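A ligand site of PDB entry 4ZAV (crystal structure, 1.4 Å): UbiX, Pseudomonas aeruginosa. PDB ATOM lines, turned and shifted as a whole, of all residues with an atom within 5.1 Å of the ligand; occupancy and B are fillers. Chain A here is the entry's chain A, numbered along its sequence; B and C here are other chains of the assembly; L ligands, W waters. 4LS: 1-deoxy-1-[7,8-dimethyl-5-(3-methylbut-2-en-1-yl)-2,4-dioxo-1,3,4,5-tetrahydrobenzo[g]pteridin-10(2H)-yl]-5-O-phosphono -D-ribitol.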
ATOM      1  N   THR A  12     -21.396 -15.138 -18.602  1.00  0.00           N
ATOM      2  CA  THR A  12     -21.942 -13.844 -18.189  1.00  0.00           C
ATOM      3  C   THR A  12     -21.182 -13.368 -16.956  1.00  0.00           C
ATOM      4  O   THR A  12     -20.374 -14.100 -16.378  1.00  0.00           O
ATOM      5  CB  THR A  12     -23.443 -13.901 -18.021  1.00  0.00           C
ATOM      6  OG1 THR A  12     -23.814 -14.721 -16.929  1.00  0.00           O
ATOM      7  CG2 THR A  12     -24.131 -14.366 -19.302  1.00  0.00           C
ATOM      8  N   GLY A  13     -21.465 -12.148 -16.567  1.00  0.00           N
ATOM      9  CA  GLY A  13     -20.603 -11.389 -15.689  1.00  0.00           C
ATOM     10  C   GLY A  13     -20.640 -11.637 -14.204  1.00  0.00           C
ATOM     11  O   GLY A  13     -20.468 -10.676 -13.422  1.00  0.00           O
ATOM     12  N   ALA A  14     -20.817 -12.867 -13.780  1.00  0.00           N
ATOM     13  CA  ALA A  14     -20.523 -13.228 -12.397  1.00  0.00           C
ATOM     14  C   ALA A  14     -19.065 -13.553 -12.218  1.00  0.00           C
ATOM     15  O   ALA A  14     -18.381 -13.956 -13.158  1.00  0.00           O
ATOM     16  CB  ALA A  14     -21.386 -14.373 -11.906  1.00  0.00           C
ATOM     17  N   SER A  15     -18.557 -13.419 -11.012  1.00  0.00           N
ATOM     18  CA  SER A  15     -17.224 -13.927 -10.680  1.00  0.00           C
ATOM     19  C   SER A  15     -17.146 -15.414 -10.997  1.00  0.00           C
ATOM     20  O   SER A  15     -18.124 -16.137 -10.797  1.00  0.00           O
ATOM     21  CB  SER A  15     -16.911 -13.534  -9.243  1.00  0.00           C
ATOM     22  OG  SER A  15     -15.562 -13.833  -8.935  1.00  0.00           O
ATOM     23  N   SER A  39     -20.861 -12.238 -22.608  1.00  0.00           N
ATOM     24  CA  SER A  39     -21.347 -10.897 -22.444  1.00  0.00           C
ATOM     25  C   SER A  39     -20.208  -9.873 -22.288  1.00  0.00           C
ATOM     26  O   SER A  39     -19.080 -10.235 -21.932  1.00  0.00           O
ATOM     27  CB  SER A  39     -22.280 -10.850 -21.229  1.00  0.00           C
ATOM     28  OG  SER A  39     -21.531 -10.887 -20.026  1.00  0.00           O
ATOM     29  N   ALA A  41     -19.967  -7.759 -19.869  1.00  0.00           N
ATOM     30  CA  ALA A  41     -19.519  -7.756 -18.471  1.00  0.00           C
ATOM     31  C   ALA A  41     -18.618  -8.928 -18.192  1.00  0.00           C
ATOM     32  O   ALA A  41     -17.650  -8.809 -17.439  1.00  0.00           O
ATOM     33  CB  ALA A  41     -20.728  -7.702 -17.531  1.00  0.00           C
ATOM     34  N   ALA A  42     -18.938 -10.079 -18.762  1.00  0.00           N
ATOM     35  CA  ALA A  42     -18.065 -11.250 -18.613  1.00  0.00           C
ATOM     36  C   ALA A  42     -16.665 -11.007 -19.167  1.00  0.00           C
ATOM     37  O   ALA A  42     -15.681 -11.540 -18.650  1.00  0.00           O
ATOM     38  CB  ALA A  42     -18.654 -12.470 -19.237  1.00  0.00           C
ATOM     39  N   LEU A  44     -15.129  -8.278 -18.981  1.00  0.00           N
ATOM     40  CA  LEU A  44     -14.400  -7.511 -17.976  1.00  0.00           C
ATOM     41  C   LEU A  44     -14.090  -8.340 -16.713  1.00  0.00           C
ATOM     42  O   LEU A  44     -13.058  -8.119 -16.051  1.00  0.00           O
ATOM     43  CB  LEU A  44     -15.139  -6.235 -17.605  1.00  0.00           C
ATOM     44  CG  LEU A  44     -14.533  -5.540 -16.440  1.00  0.00           C
ATOM     45  CD1 LEU A  44     -13.183  -4.924 -16.732  1.00  0.00           C
ATOM     46  CD2 LEU A  44     -15.474  -4.430 -15.998  1.00  0.00           C
ATOM     47  N   VAL A  45     -14.950  -9.317 -16.395  1.00  0.00           N
ATOM     48  CA  VAL A  45     -14.613 -10.285 -15.339  1.00  0.00           C
ATOM     49  C   VAL A  45     -13.339 -11.062 -15.772  1.00  0.00           C
ATOM     50  O   VAL A  45     -12.442 -11.265 -14.913  1.00  0.00           O
ATOM     51  CB  VAL A  45     -15.779 -11.215 -15.007  1.00  0.00           C
ATOM     52  CG1 VAL A  45     -15.336 -12.225 -13.958  1.00  0.00           C
ATOM     53  CG2 VAL A  45     -17.015 -10.440 -14.493  1.00  0.00           C
ATOM     54  N   THR A  48     -10.228  -9.185 -15.353  1.00  0.00           N
ATOM     55  CA  THR A  48      -9.949  -8.828 -13.946  1.00  0.00           C
ATOM     56  C   THR A  48      -9.366 -10.063 -13.210  1.00  0.00           C
ATOM     57  O   THR A  48      -8.498  -9.920 -12.359  1.00  0.00           O
ATOM     58  CB  THR A  48     -11.288  -8.391 -13.276  1.00  0.00           C
ATOM     59  OG1 THR A  48     -11.768  -7.207 -13.940  1.00  0.00           O
ATOM     60  CG2 THR A  48     -11.093  -8.133 -11.788  1.00  0.00           C
ATOM     61  N   GLU A  49      -9.916 -11.242 -13.504  1.00  0.00           N
ATOM     62  CA  GLU A  49      -9.687 -12.473 -12.703  1.00  0.00           C
ATOM     63  C   GLU A  49      -8.683 -13.422 -13.268  1.00  0.00           C
ATOM     64  O   GLU A  49      -8.270 -14.314 -12.562  1.00  0.00           O
ATOM     65  CB  GLU A  49     -11.010 -13.307 -12.546  1.00  0.00           C
ATOM     66  CG  GLU A  49     -11.998 -12.537 -11.788  1.00  0.00           C
ATOM     67  CD  GLU A  49     -13.234 -13.356 -11.360  1.00  0.00           C
ATOM     68  OE1 GLU A  49     -13.531 -14.479 -11.891  1.00  0.00           O
ATOM     69  OE2 GLU A  49     -13.942 -12.750 -10.494  1.00  0.00           O
ATOM     70  N   CYS A 103     -23.205 -17.546 -14.368  1.00  0.00           N
ATOM     71  CA  CYS A 103     -24.474 -16.902 -14.591  1.00  0.00           C
ATOM     72  C   CYS A 103     -24.643 -15.745 -13.629  1.00  0.00           C
ATOM     73  O   CYS A 103     -24.820 -15.942 -12.447  1.00  0.00           O
ATOM     74  CB  CYS A 103     -25.615 -17.899 -14.428  1.00  0.00           C
ATOM     75  SG  CYS A 103     -27.230 -17.168 -14.889  1.00  0.00           S
ATOM     76  N   SER A 104     -24.567 -14.525 -14.154  1.00  0.00           N
ATOM     77  CA  SER A 104     -24.793 -13.353 -13.332  1.00  0.00           C
ATOM     78  C   SER A 104     -26.230 -13.329 -12.795  1.00  0.00           C
ATOM     79  O   SER A 104     -27.148 -13.924 -13.367  1.00  0.00           O
ATOM     80  CB  SER A 104     -24.562 -12.067 -14.126  1.00  0.00           C
ATOM     81  OG  SER A 104     -25.599 -11.868 -15.047  1.00  0.00           O
ATOM     82  N   THR A 105     -26.447 -12.547 -11.735  1.00  0.00           N
ATOM     83  CA  THR A 105     -27.805 -12.373 -11.260  1.00  0.00           C
ATOM     84  C   THR A 105     -28.688 -11.672 -12.319  1.00  0.00           C
ATOM     85  O   THR A 105     -29.902 -11.969 -12.392  1.00  0.00           O
ATOM     86  CB  THR A 105     -27.881 -11.632  -9.916  1.00  0.00           C
ATOM     87  OG1 THR A 105     -27.350 -10.339 -10.036  1.00  0.00           O
ATOM     88  CG2 THR A 105     -27.143 -12.366  -8.849  1.00  0.00           C
ATOM     89  N   GLY A 106     -28.075 -10.805 -13.128  1.00  0.00           N
ATOM     90  CA  GLY A 106     -28.844 -10.157 -14.155  1.00  0.00           C
ATOM     91  C   GLY A 106     -29.298 -11.081 -15.272  1.00  0.00           C
ATOM     92  O   GLY A 106     -30.392 -10.959 -15.792  1.00  0.00           O
ATOM     93  N   THR A 107     -28.406 -12.003 -15.639  1.00  0.00           N
ATOM     94  CA  THR A 107     -28.798 -12.993 -16.674  1.00  0.00           C
ATOM     95  C   THR A 107     -29.795 -13.979 -16.098  1.00  0.00           C
ATOM     96  O   THR A 107     -30.747 -14.370 -16.755  1.00  0.00           O
ATOM     97  CB  THR A 107     -27.569 -13.668 -17.290  1.00  0.00           C
ATOM     98  OG1 THR A 107     -26.864 -12.712 -18.110  1.00  0.00           O
ATOM     99  CG2 THR A 107     -27.968 -14.845 -18.132  1.00  0.00           C
ATOM    100  N   ARG A 139     -23.119 -17.396  -9.288  1.00  0.00           N
ATOM    101  CA  ARG A 139     -22.072 -17.160  -8.246  1.00  0.00           C
ATOM    102  C   ARG A 139     -22.451 -15.862  -7.600  1.00  0.00           C
ATOM    103  O   ARG A 139     -22.292 -14.805  -8.190  1.00  0.00           O
ATOM    104  CB  ARG A 139     -20.702 -17.098  -8.906  1.00  0.00           C
ATOM    105  CG  ARG A 139     -19.526 -17.302  -7.963  1.00  0.00           C
ATOM    106  CD  ARG A 139     -19.580 -16.554  -6.629  1.00  0.00           C
ATOM    107  NE  ARG A 139     -19.577 -15.126  -6.740  1.00  0.00           N
ATOM    108  CZ  ARG A 139     -19.698 -14.306  -5.709  1.00  0.00           C
ATOM    109  NH1 ARG A 139     -19.677 -14.777  -4.458  1.00  0.00           N
ATOM    110  NH2 ARG A 139     -19.841 -13.024  -5.959  1.00  0.00           N
ATOM    111  N   GLU A 140     -23.040 -15.969  -6.406  1.00  0.00           N
ATOM    112  CA  GLU A 140     -23.446 -14.797  -5.657  1.00  0.00           C
ATOM    113  C   GLU A 140     -23.578 -15.257  -4.219  1.00  0.00           C
ATOM    114  O   GLU A 140     -23.843 -16.397  -3.909  1.00  0.00           O
ATOM    115  CB  GLU A 140     -24.798 -14.231  -6.221  1.00  0.00           C
ATOM    116  CG  GLU A 140     -25.278 -12.930  -5.516  1.00  0.00           C
ATOM    117  CD  GLU A 140     -24.294 -11.813  -5.655  1.00  0.00           C
ATOM    118  OE1 GLU A 140     -23.360 -11.788  -4.780  1.00  0.00           O
ATOM    119  OE2 GLU A 140     -24.400 -11.002  -6.614  1.00  0.00           O
ATOM    120  N   TRP B  84     -18.366  -1.058 -12.975  1.00  0.00           N
ATOM    121  CA  TRP B  84     -18.433  -2.140 -12.032  1.00  0.00           C
ATOM    122  C   TRP B  84     -17.338  -2.080 -10.956  1.00  0.00           C
ATOM    123  O   TRP B  84     -17.367  -2.844  -9.990  1.00  0.00           O
ATOM    124  CB  TRP B  84     -18.403  -3.498 -12.763  1.00  0.00           C
ATOM    125  CG  TRP B  84     -19.428  -3.556 -13.838  1.00  0.00           C
ATOM    126  CD1 TRP B  84     -19.169  -3.704 -15.182  1.00  0.00           C
ATOM    127  CD2 TRP B  84     -20.848  -3.452 -13.733  1.00  0.00           C
ATOM    128  NE1 TRP B  84     -20.311  -3.670 -15.890  1.00  0.00           N
ATOM    129  CE2 TRP B  84     -21.362  -3.485 -15.031  1.00  0.00           C
ATOM    130  CE3 TRP B  84     -21.752  -3.271 -12.681  1.00  0.00           C
ATOM    131  CZ2 TRP B  84     -22.704  -3.378 -15.284  1.00  0.00           C
ATOM    132  CZ3 TRP B  84     -23.083  -3.155 -12.944  1.00  0.00           C
ATOM    133  CH2 TRP B  84     -23.560  -3.213 -14.231  1.00  0.00           C
ATOM    134  N   MET B  85     -16.301  -1.283 -11.157  1.00  0.00           N
ATOM    135  CA  MET B  85     -15.297  -1.152 -10.064  1.00  0.00           C
ATOM    136  C   MET B  85     -15.664  -0.110  -9.031  1.00  0.00           C
ATOM    137  O   MET B  85     -14.884   0.146  -8.104  1.00  0.00           O
ATOM    138  CB  MET B  85     -13.932  -0.866 -10.669  1.00  0.00           C
ATOM    139  CG  MET B  85     -13.200  -2.133 -11.160  1.00  0.00           C
ATOM    140  SD  MET B  85     -14.145  -3.278 -12.221  1.00  0.00           S
ATOM    141  CE  MET B  85     -12.971  -4.604 -12.474  1.00  0.00           C
ATOM    142  N   ALA B  89     -21.378  -1.607  -6.688  1.00  0.00           N
ATOM    143  CA  ALA B  89     -21.541  -2.823  -7.505  1.00  0.00           C
ATOM    144  C   ALA B  89     -21.342  -4.142  -6.733  1.00  0.00           C
ATOM    145  O   ALA B  89     -21.732  -5.203  -7.257  1.00  0.00           O
ATOM    146  CB  ALA B  89     -20.577  -2.781  -8.671  1.00  0.00           C
ATOM    147  N   SER B  90     -20.702  -4.085  -5.554  1.00  0.00           N
ATOM    148  CA  SER B  90     -20.407  -5.285  -4.783  1.00  0.00           C
ATOM    149  C   SER B  90     -20.911  -5.156  -3.374  1.00  0.00           C
ATOM    150  O   SER B  90     -20.803  -4.089  -2.775  1.00  0.00           O
ATOM    151  CB  SER B  90     -18.898  -5.537  -4.704  1.00  0.00           C
ATOM    152  OG  SER B  90     -18.592  -6.636  -3.906  1.00  0.00           O
ATOM    153  N   CYS B 116     -30.458  -5.920 -13.051  1.00  0.00           N
ATOM    154  CA  CYS B 116     -29.025  -5.559 -12.976  1.00  0.00           C
ATOM    155  C   CYS B 116     -28.367  -5.151 -14.325  1.00  0.00           C
ATOM    156  O   CYS B 116     -27.202  -5.468 -14.550  1.00  0.00           O
ATOM    157  CB  CYS B 116     -28.178  -6.707 -12.368  1.00  0.00           C
ATOM    158  SG  CYS B 116     -28.470  -7.123 -10.693  1.00  0.00           S
ATOM    159  N   ASN B 117     -29.048  -4.329 -15.143  1.00  0.00           N
ATOM    160  CA  ASN B 117     -28.515  -3.945 -16.434  1.00  0.00           C
ATOM    161  C   ASN B 117     -27.545  -2.764 -16.484  1.00  0.00           C
ATOM    162  O   ASN B 117     -26.882  -2.511 -17.469  1.00  0.00           O
ATOM    163  CB  ASN B 117     -29.612  -3.751 -17.415  1.00  0.00           C
ATOM    164  CG  ASN B 117     -30.126  -5.090 -17.975  1.00  0.00           C
ATOM    165  OD1 ASN B 117     -29.306  -6.021 -18.272  1.00  0.00           O
ATOM    166  ND2 ASN B 117     -31.458  -5.212 -18.093  1.00  0.00           N
ATOM    167  N   ASN B 118     -27.404  -2.094 -15.346  1.00  0.00           N
ATOM    168  CA  ASN B 118     -26.485  -0.974 -15.225  1.00  0.00           C
ATOM    169  C   ASN B 118     -26.155  -0.854 -13.742  1.00  0.00           C
ATOM    170  O   ASN B 118     -26.676  -1.620 -12.903  1.00  0.00           O
ATOM    171  CB  ASN B 118     -27.145   0.315 -15.773  1.00  0.00           C
ATOM    172  CG  ASN B 118     -28.463   0.599 -15.100  1.00  0.00           C
ATOM    173  OD1 ASN B 118     -28.617   0.590 -13.892  1.00  0.00           O
ATOM    174  ND2 ASN B 118     -29.467   0.755 -15.909  1.00  0.00           N
ATOM    175  N   ARG B 122     -27.838  -2.772 -10.446  1.00  0.00           N
ATOM    176  CA  ARG B 122     -26.982  -3.656  -9.673  1.00  0.00           C
ATOM    177  C   ARG B 122     -26.808  -3.176  -8.271  1.00  0.00           C
ATOM    178  O   ARG B 122     -26.821  -3.972  -7.313  1.00  0.00           O
ATOM    179  CB  ARG B 122     -25.641  -3.842 -10.369  1.00  0.00           C
ATOM    180  CG  ARG B 122     -24.600  -4.608  -9.586  1.00  0.00           C
ATOM    181  CD  ARG B 122     -25.003  -6.065  -9.301  1.00  0.00           C
ATOM    182  NE  ARG B 122     -23.877  -6.641  -8.560  1.00  0.00           N
ATOM    183  CZ  ARG B 122     -23.884  -7.869  -8.044  1.00  0.00           C
ATOM    184  NH1 ARG B 122     -24.906  -8.686  -8.232  1.00  0.00           N
ATOM    185  NH2 ARG B 122     -22.856  -8.251  -7.289  1.00  0.00           N
ATOM    186  N   TYR C 169     -12.703 -12.549  -7.487  1.00  0.00           N
ATOM    187  CA  TYR C 169     -12.345 -11.242  -7.960  1.00  0.00           C
ATOM    188  C   TYR C 169     -11.181 -10.581  -7.176  1.00  0.00           C
ATOM    189  O   TYR C 169     -10.730  -9.484  -7.512  1.00  0.00           O
ATOM    190  CB  TYR C 169     -13.562 -10.320  -8.029  1.00  0.00           C
ATOM    191  CG  TYR C 169     -14.439 -10.220  -6.814  1.00  0.00           C
ATOM    192  CD1 TYR C 169     -14.161  -9.346  -5.778  1.00  0.00           C
ATOM    193  CD2 TYR C 169     -15.597 -10.954  -6.727  1.00  0.00           C
ATOM    194  CE1 TYR C 169     -15.020  -9.212  -4.724  1.00  0.00           C
ATOM    195  CE2 TYR C 169     -16.469 -10.838  -5.663  1.00  0.00           C
ATOM    196  CZ  TYR C 169     -16.200  -9.964  -4.687  1.00  0.00           C
ATOM    197  OH  TYR C 169     -17.058  -9.739  -3.645  1.00  0.00           O
ATOM    198  N   TRP C 200     -14.682  -3.357  -1.564  1.00  0.00           N
ATOM    199  CA  TRP C 200     -14.636  -3.108  -2.979  1.00  0.00           C
ATOM    200  C   TRP C 200     -14.794  -1.636  -3.353  1.00  0.00           C
ATOM    201  O   TRP C 200     -15.733  -0.999  -2.901  1.00  0.00           O
ATOM    202  CB  TRP C 200     -15.753  -3.874  -3.710  1.00  0.00           C
ATOM    203  CG  TRP C 200     -15.745  -3.783  -5.193  1.00  0.00           C
ATOM    204  CD1 TRP C 200     -16.567  -3.034  -5.992  1.00  0.00           C
ATOM    205  CD2 TRP C 200     -14.867  -4.480  -6.044  1.00  0.00           C
ATOM    206  NE1 TRP C 200     -16.254  -3.228  -7.293  1.00  0.00           N
ATOM    207  CE2 TRP C 200     -15.204  -4.133  -7.357  1.00  0.00           C
ATOM    208  CE3 TRP C 200     -13.833  -5.398  -5.838  1.00  0.00           C
ATOM    209  CZ2 TRP C 200     -14.534  -4.679  -8.455  1.00  0.00           C
ATOM    210  CZ3 TRP C 200     -13.158  -5.893  -6.907  1.00  0.00           C
ATOM    211  CH2 TRP C 200     -13.482  -5.516  -8.191  1.00  0.00           C
HETATM  212  C4A 4LS L   1     -20.361 -10.577  -9.781  1.00  0.00           C
HETATM  213  CAA 4LS L   1     -16.786  -7.421  -7.582  1.00  0.00           C
HETATM  214  CAC 4LS L   1     -16.937  -6.640 -13.423  1.00  0.00           C
HETATM  215  CAD 4LS L   1     -15.089  -8.170 -11.650  1.00  0.00           C
HETATM  216  OAL 4LS L   1     -25.421 -10.643 -17.242  1.00  0.00           O
HETATM  217  PBK 4LS L   1     -24.375  -9.755 -17.874  1.00  0.00           P
HETATM  218  OAM 4LS L   1     -24.778  -9.209 -19.233  1.00  0.00           O
HETATM  219  OAH 4LS L   1     -23.031 -10.392 -17.910  1.00  0.00           O
HETATM  220  OAV 4LS L   1     -24.315  -8.455 -16.981  1.00  0.00           O
HETATM  221  CAR 4LS L   1     -23.966  -8.520 -15.584  1.00  0.00           C
HETATM  222  CBF 4LS L   1     -23.707  -7.141 -15.079  1.00  0.00           C
HETATM  223  OAI 4LS L   1     -24.732  -6.248 -15.404  1.00  0.00           O
HETATM  224  CBH 4LS L   1     -23.286  -7.104 -13.663  1.00  0.00           C
HETATM  225  OAK 4LS L   1     -24.455  -6.986 -12.813  1.00  0.00           O
HETATM  226  CBG 4LS L   1     -22.295  -8.000 -13.138  1.00  0.00           C
HETATM  227  OAJ 4LS L   1     -21.268  -8.234 -14.107  1.00  0.00           O
HETATM  228  CAS 4LS L   1     -21.775  -7.734 -11.755  1.00  0.00           C
HETATM  229  N10 4LS L   1     -20.822  -8.684 -11.169  1.00  0.00           N
HETATM  230  C9A 4LS L   1     -19.430  -8.524 -11.341  1.00  0.00           C
HETATM  231  C9  4LS L   1     -18.871  -7.633 -12.302  1.00  0.00           C
HETATM  232  C8  4LS L   1     -17.462  -7.494 -12.412  1.00  0.00           C
HETATM  233  C7  4LS L   1     -16.585  -8.280 -11.591  1.00  0.00           C
HETATM  234  C6  4LS L   1     -17.160  -9.149 -10.682  1.00  0.00           C
HETATM  235  C5A 4LS L   1     -18.538  -9.271 -10.531  1.00  0.00           C
HETATM  236  N5  4LS L   1     -19.013 -10.142  -9.579  1.00  0.00           N
HETATM  237  CAQ 4LS L   1     -18.794  -9.708  -8.194  1.00  0.00           C
HETATM  238  CAN 4LS L   1     -19.135  -8.185  -8.162  1.00  0.00           C
HETATM  239  CAW 4LS L   1     -18.167  -7.173  -8.079  1.00  0.00           C
HETATM  240  CAB 4LS L   1     -18.495  -5.792  -8.564  1.00  0.00           C
HETATM  241  C11 4LS L   1     -21.252  -9.809 -10.532  1.00  0.00           C
HETATM  242  N1  4LS L   1     -22.570 -10.236 -10.703  1.00  0.00           N
HETATM  243  C2  4LS L   1     -22.983 -11.404 -10.144  1.00  0.00           C
HETATM  244  O2  4LS L   1     -24.124 -11.864 -10.303  1.00  0.00           O
HETATM  245  N3  4LS L   1     -22.084 -12.104  -9.435  1.00  0.00           N
HETATM  246  C4  4LS L   1     -20.770 -11.786  -9.221  1.00  0.00           C
HETATM  247  O4  4LS L   1     -20.043 -12.598  -8.622  1.00  0.00           O
HETATM  248  O   HOH W   1     -26.524  -7.061 -19.157  1.00  0.00           O
HETATM  249  O   HOH W   2     -24.722 -15.008  -9.954  1.00  0.00           O
HETATM  250  O   HOH W   3     -25.342  -9.418 -11.805  1.00  0.00           O
HETATM  251  O   HOH W   4     -22.940  -7.498 -20.301  1.00  0.00           O
HETATM  252  O   HOH W   5     -27.282  -7.969 -16.218  1.00  0.00           O
HETATM  253  O   HOH W   6     -25.148  -5.033 -17.688  1.00  0.00           O
HETATM  254  O   HOH W   7     -28.242  -9.888 -18.283  1.00  0.00           O
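Water W6 lies within hydrogen-bond range of an oxygen (OAI) of the ligand (2.6 Å) and the backbone carbonyl oxygen of Asn 117 of chain B (3.1 Å). Water W4 bridges OAM of the ligand and N of Ala 41. Water W1 bridges an oxygen (OAM) of the ligand (2.8 Å) and the side-chain amide oxygen (OD1) of Asn 117 of chain B (3.1 Å). Water W3 lies within hydrogen-bond range of an oxygen (OAK) of the ligand, the side-chain hydroxyl of Thr 105 and the backbone NH of Gly 106. Water W7 lies within hydrogen-bond range of an oxygen (OAL) of the ligand (3.1 Å), the side-chain hydroxyl (OG1) of Thr 107 (3.1 Å) and the backbone carbonyl oxygen (O) of Gly 106 (3.5 Å). Water W2 lies within hydrogen-bond range of the backbone carbonyl oxygen (O) of Cys 103 (2.7 Å), the backbone NH (N) of Arg 139 (3.0 Å), an oxygen (O2) of the ligand (3.2 Å) and the backbone NH (N) of Thr 105 (3.5 Å).
Thr 12 touches the ligand (CB to OAH, 3.5 Å). Ala 14 touches the ligand (CB to N3, 3.4 Å). Ala 41 touches the ligand. CD2 of Leu 44 touches CAC of the ligand, 3.7 Å away. CG2 of Val 45 touches C8 of the ligand, at 3.6 Å. Thr 48 touches the ligand (CG2 to CAD, 3.999 Å). Glu 140 touches the ligand (OE2 to O2, 3.8 Å). CH2 of Trp 84 of chain B touches OAI of the ligand, at 3.5 Å. Ala 89 of chain B touches the ligand. CB of Ser 90 of chain B touches CAW of the ligand (3.8 Å). Arg 122 of chain B touches the ligand. Tyr 169 of chain C touches the ligand (CE2 to CAQ, 3.6 Å). Trp 200 of chain C touches the ligand. 21 residues have an atom within 4 Å of the ligand: Thr 12, Gly 13, Ala 14, Ser 15, Ser 39, Ala 41, Leu 44, Val 45, Thr 48, Ser 104, Thr 105, Thr 107, Arg 139, Glu 140, Trp 84 of chain B, Ala 89 of chain B, Ser 90 of chain B, Cys 116 of chain B, Arg 122 of chain B, Tyr 169 of chain C and Trp 200 of chain C.
An oxygen (OAL) of the ligand lies within hydrogen-bond range of the side-chain hydroxyl (OG) of Ser 104, 2.5 Å away. An oxygen (OAH) of the ligand is in hydrogen-bond range of the side-chain hydroxyl of Ser 39 (2.6 Å). An oxygen (OAH) of the ligand lies within hydrogen-bond range of the backbone NH (N) of Gly 13. OAJ of the ligand lies within hydrogen-bond range of O of Gly 13. OG1 of Thr 107 lies within hydrogen-bond range of OAL of the ligand. O of Arg 139 sits at hydrogen-bond distance from N3 of the ligand (3.0 Å). NH2 of Arg 139 sits at hydrogen-bond distance from O4 of the ligand. An oxygen (OAI) of the ligand sits at hydrogen-bond distance from the backbone carbonyl oxygen of Cys 116 of chain B, 2.7 Å away. O2 of the ligand sits at hydrogen-bond distance from N of Thr 105. An oxygen (O4) of the ligand sits at hydrogen-bond distance from the backbone NH of Ser 15 (2.9 Å).
The side-chain hydroxyl (OG) of Ser 104 sits at hydrogen-bond distance from the backbone NH (N) of Thr 107 (2.9 Å). OG of Ser 104 lies close to N of Gly 106 (3.3 Å). The side-chain hydroxyl of Ser 39 sits at hydrogen-bond distance from the backbone NH of Ala 42 (3.0 Å). OE1 of Glu 140 lies within salt-bridge range of NH2 of Arg 139 (3.9 Å). The side-chain hydroxyl of Thr 105 is in hydrogen-bond range of the guanidinium group of Arg 122 of chain B (3.5 Å). OE2 of Glu 49 sits at hydrogen-bond distance from OG of Ser 15 (2.5 Å). The indole nitrogen (NE1) of Trp 200 of chain C lies within hydrogen-bond range of the backbone carbonyl oxygen (O) of Trp 84 of chain B, 2.9 Å away. The side-chain carboxylate (OE2) of Glu 49 lies within hydrogen-bond range of the backbone NH (N) of Tyr 169 of chain C, at 3.3 Å.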
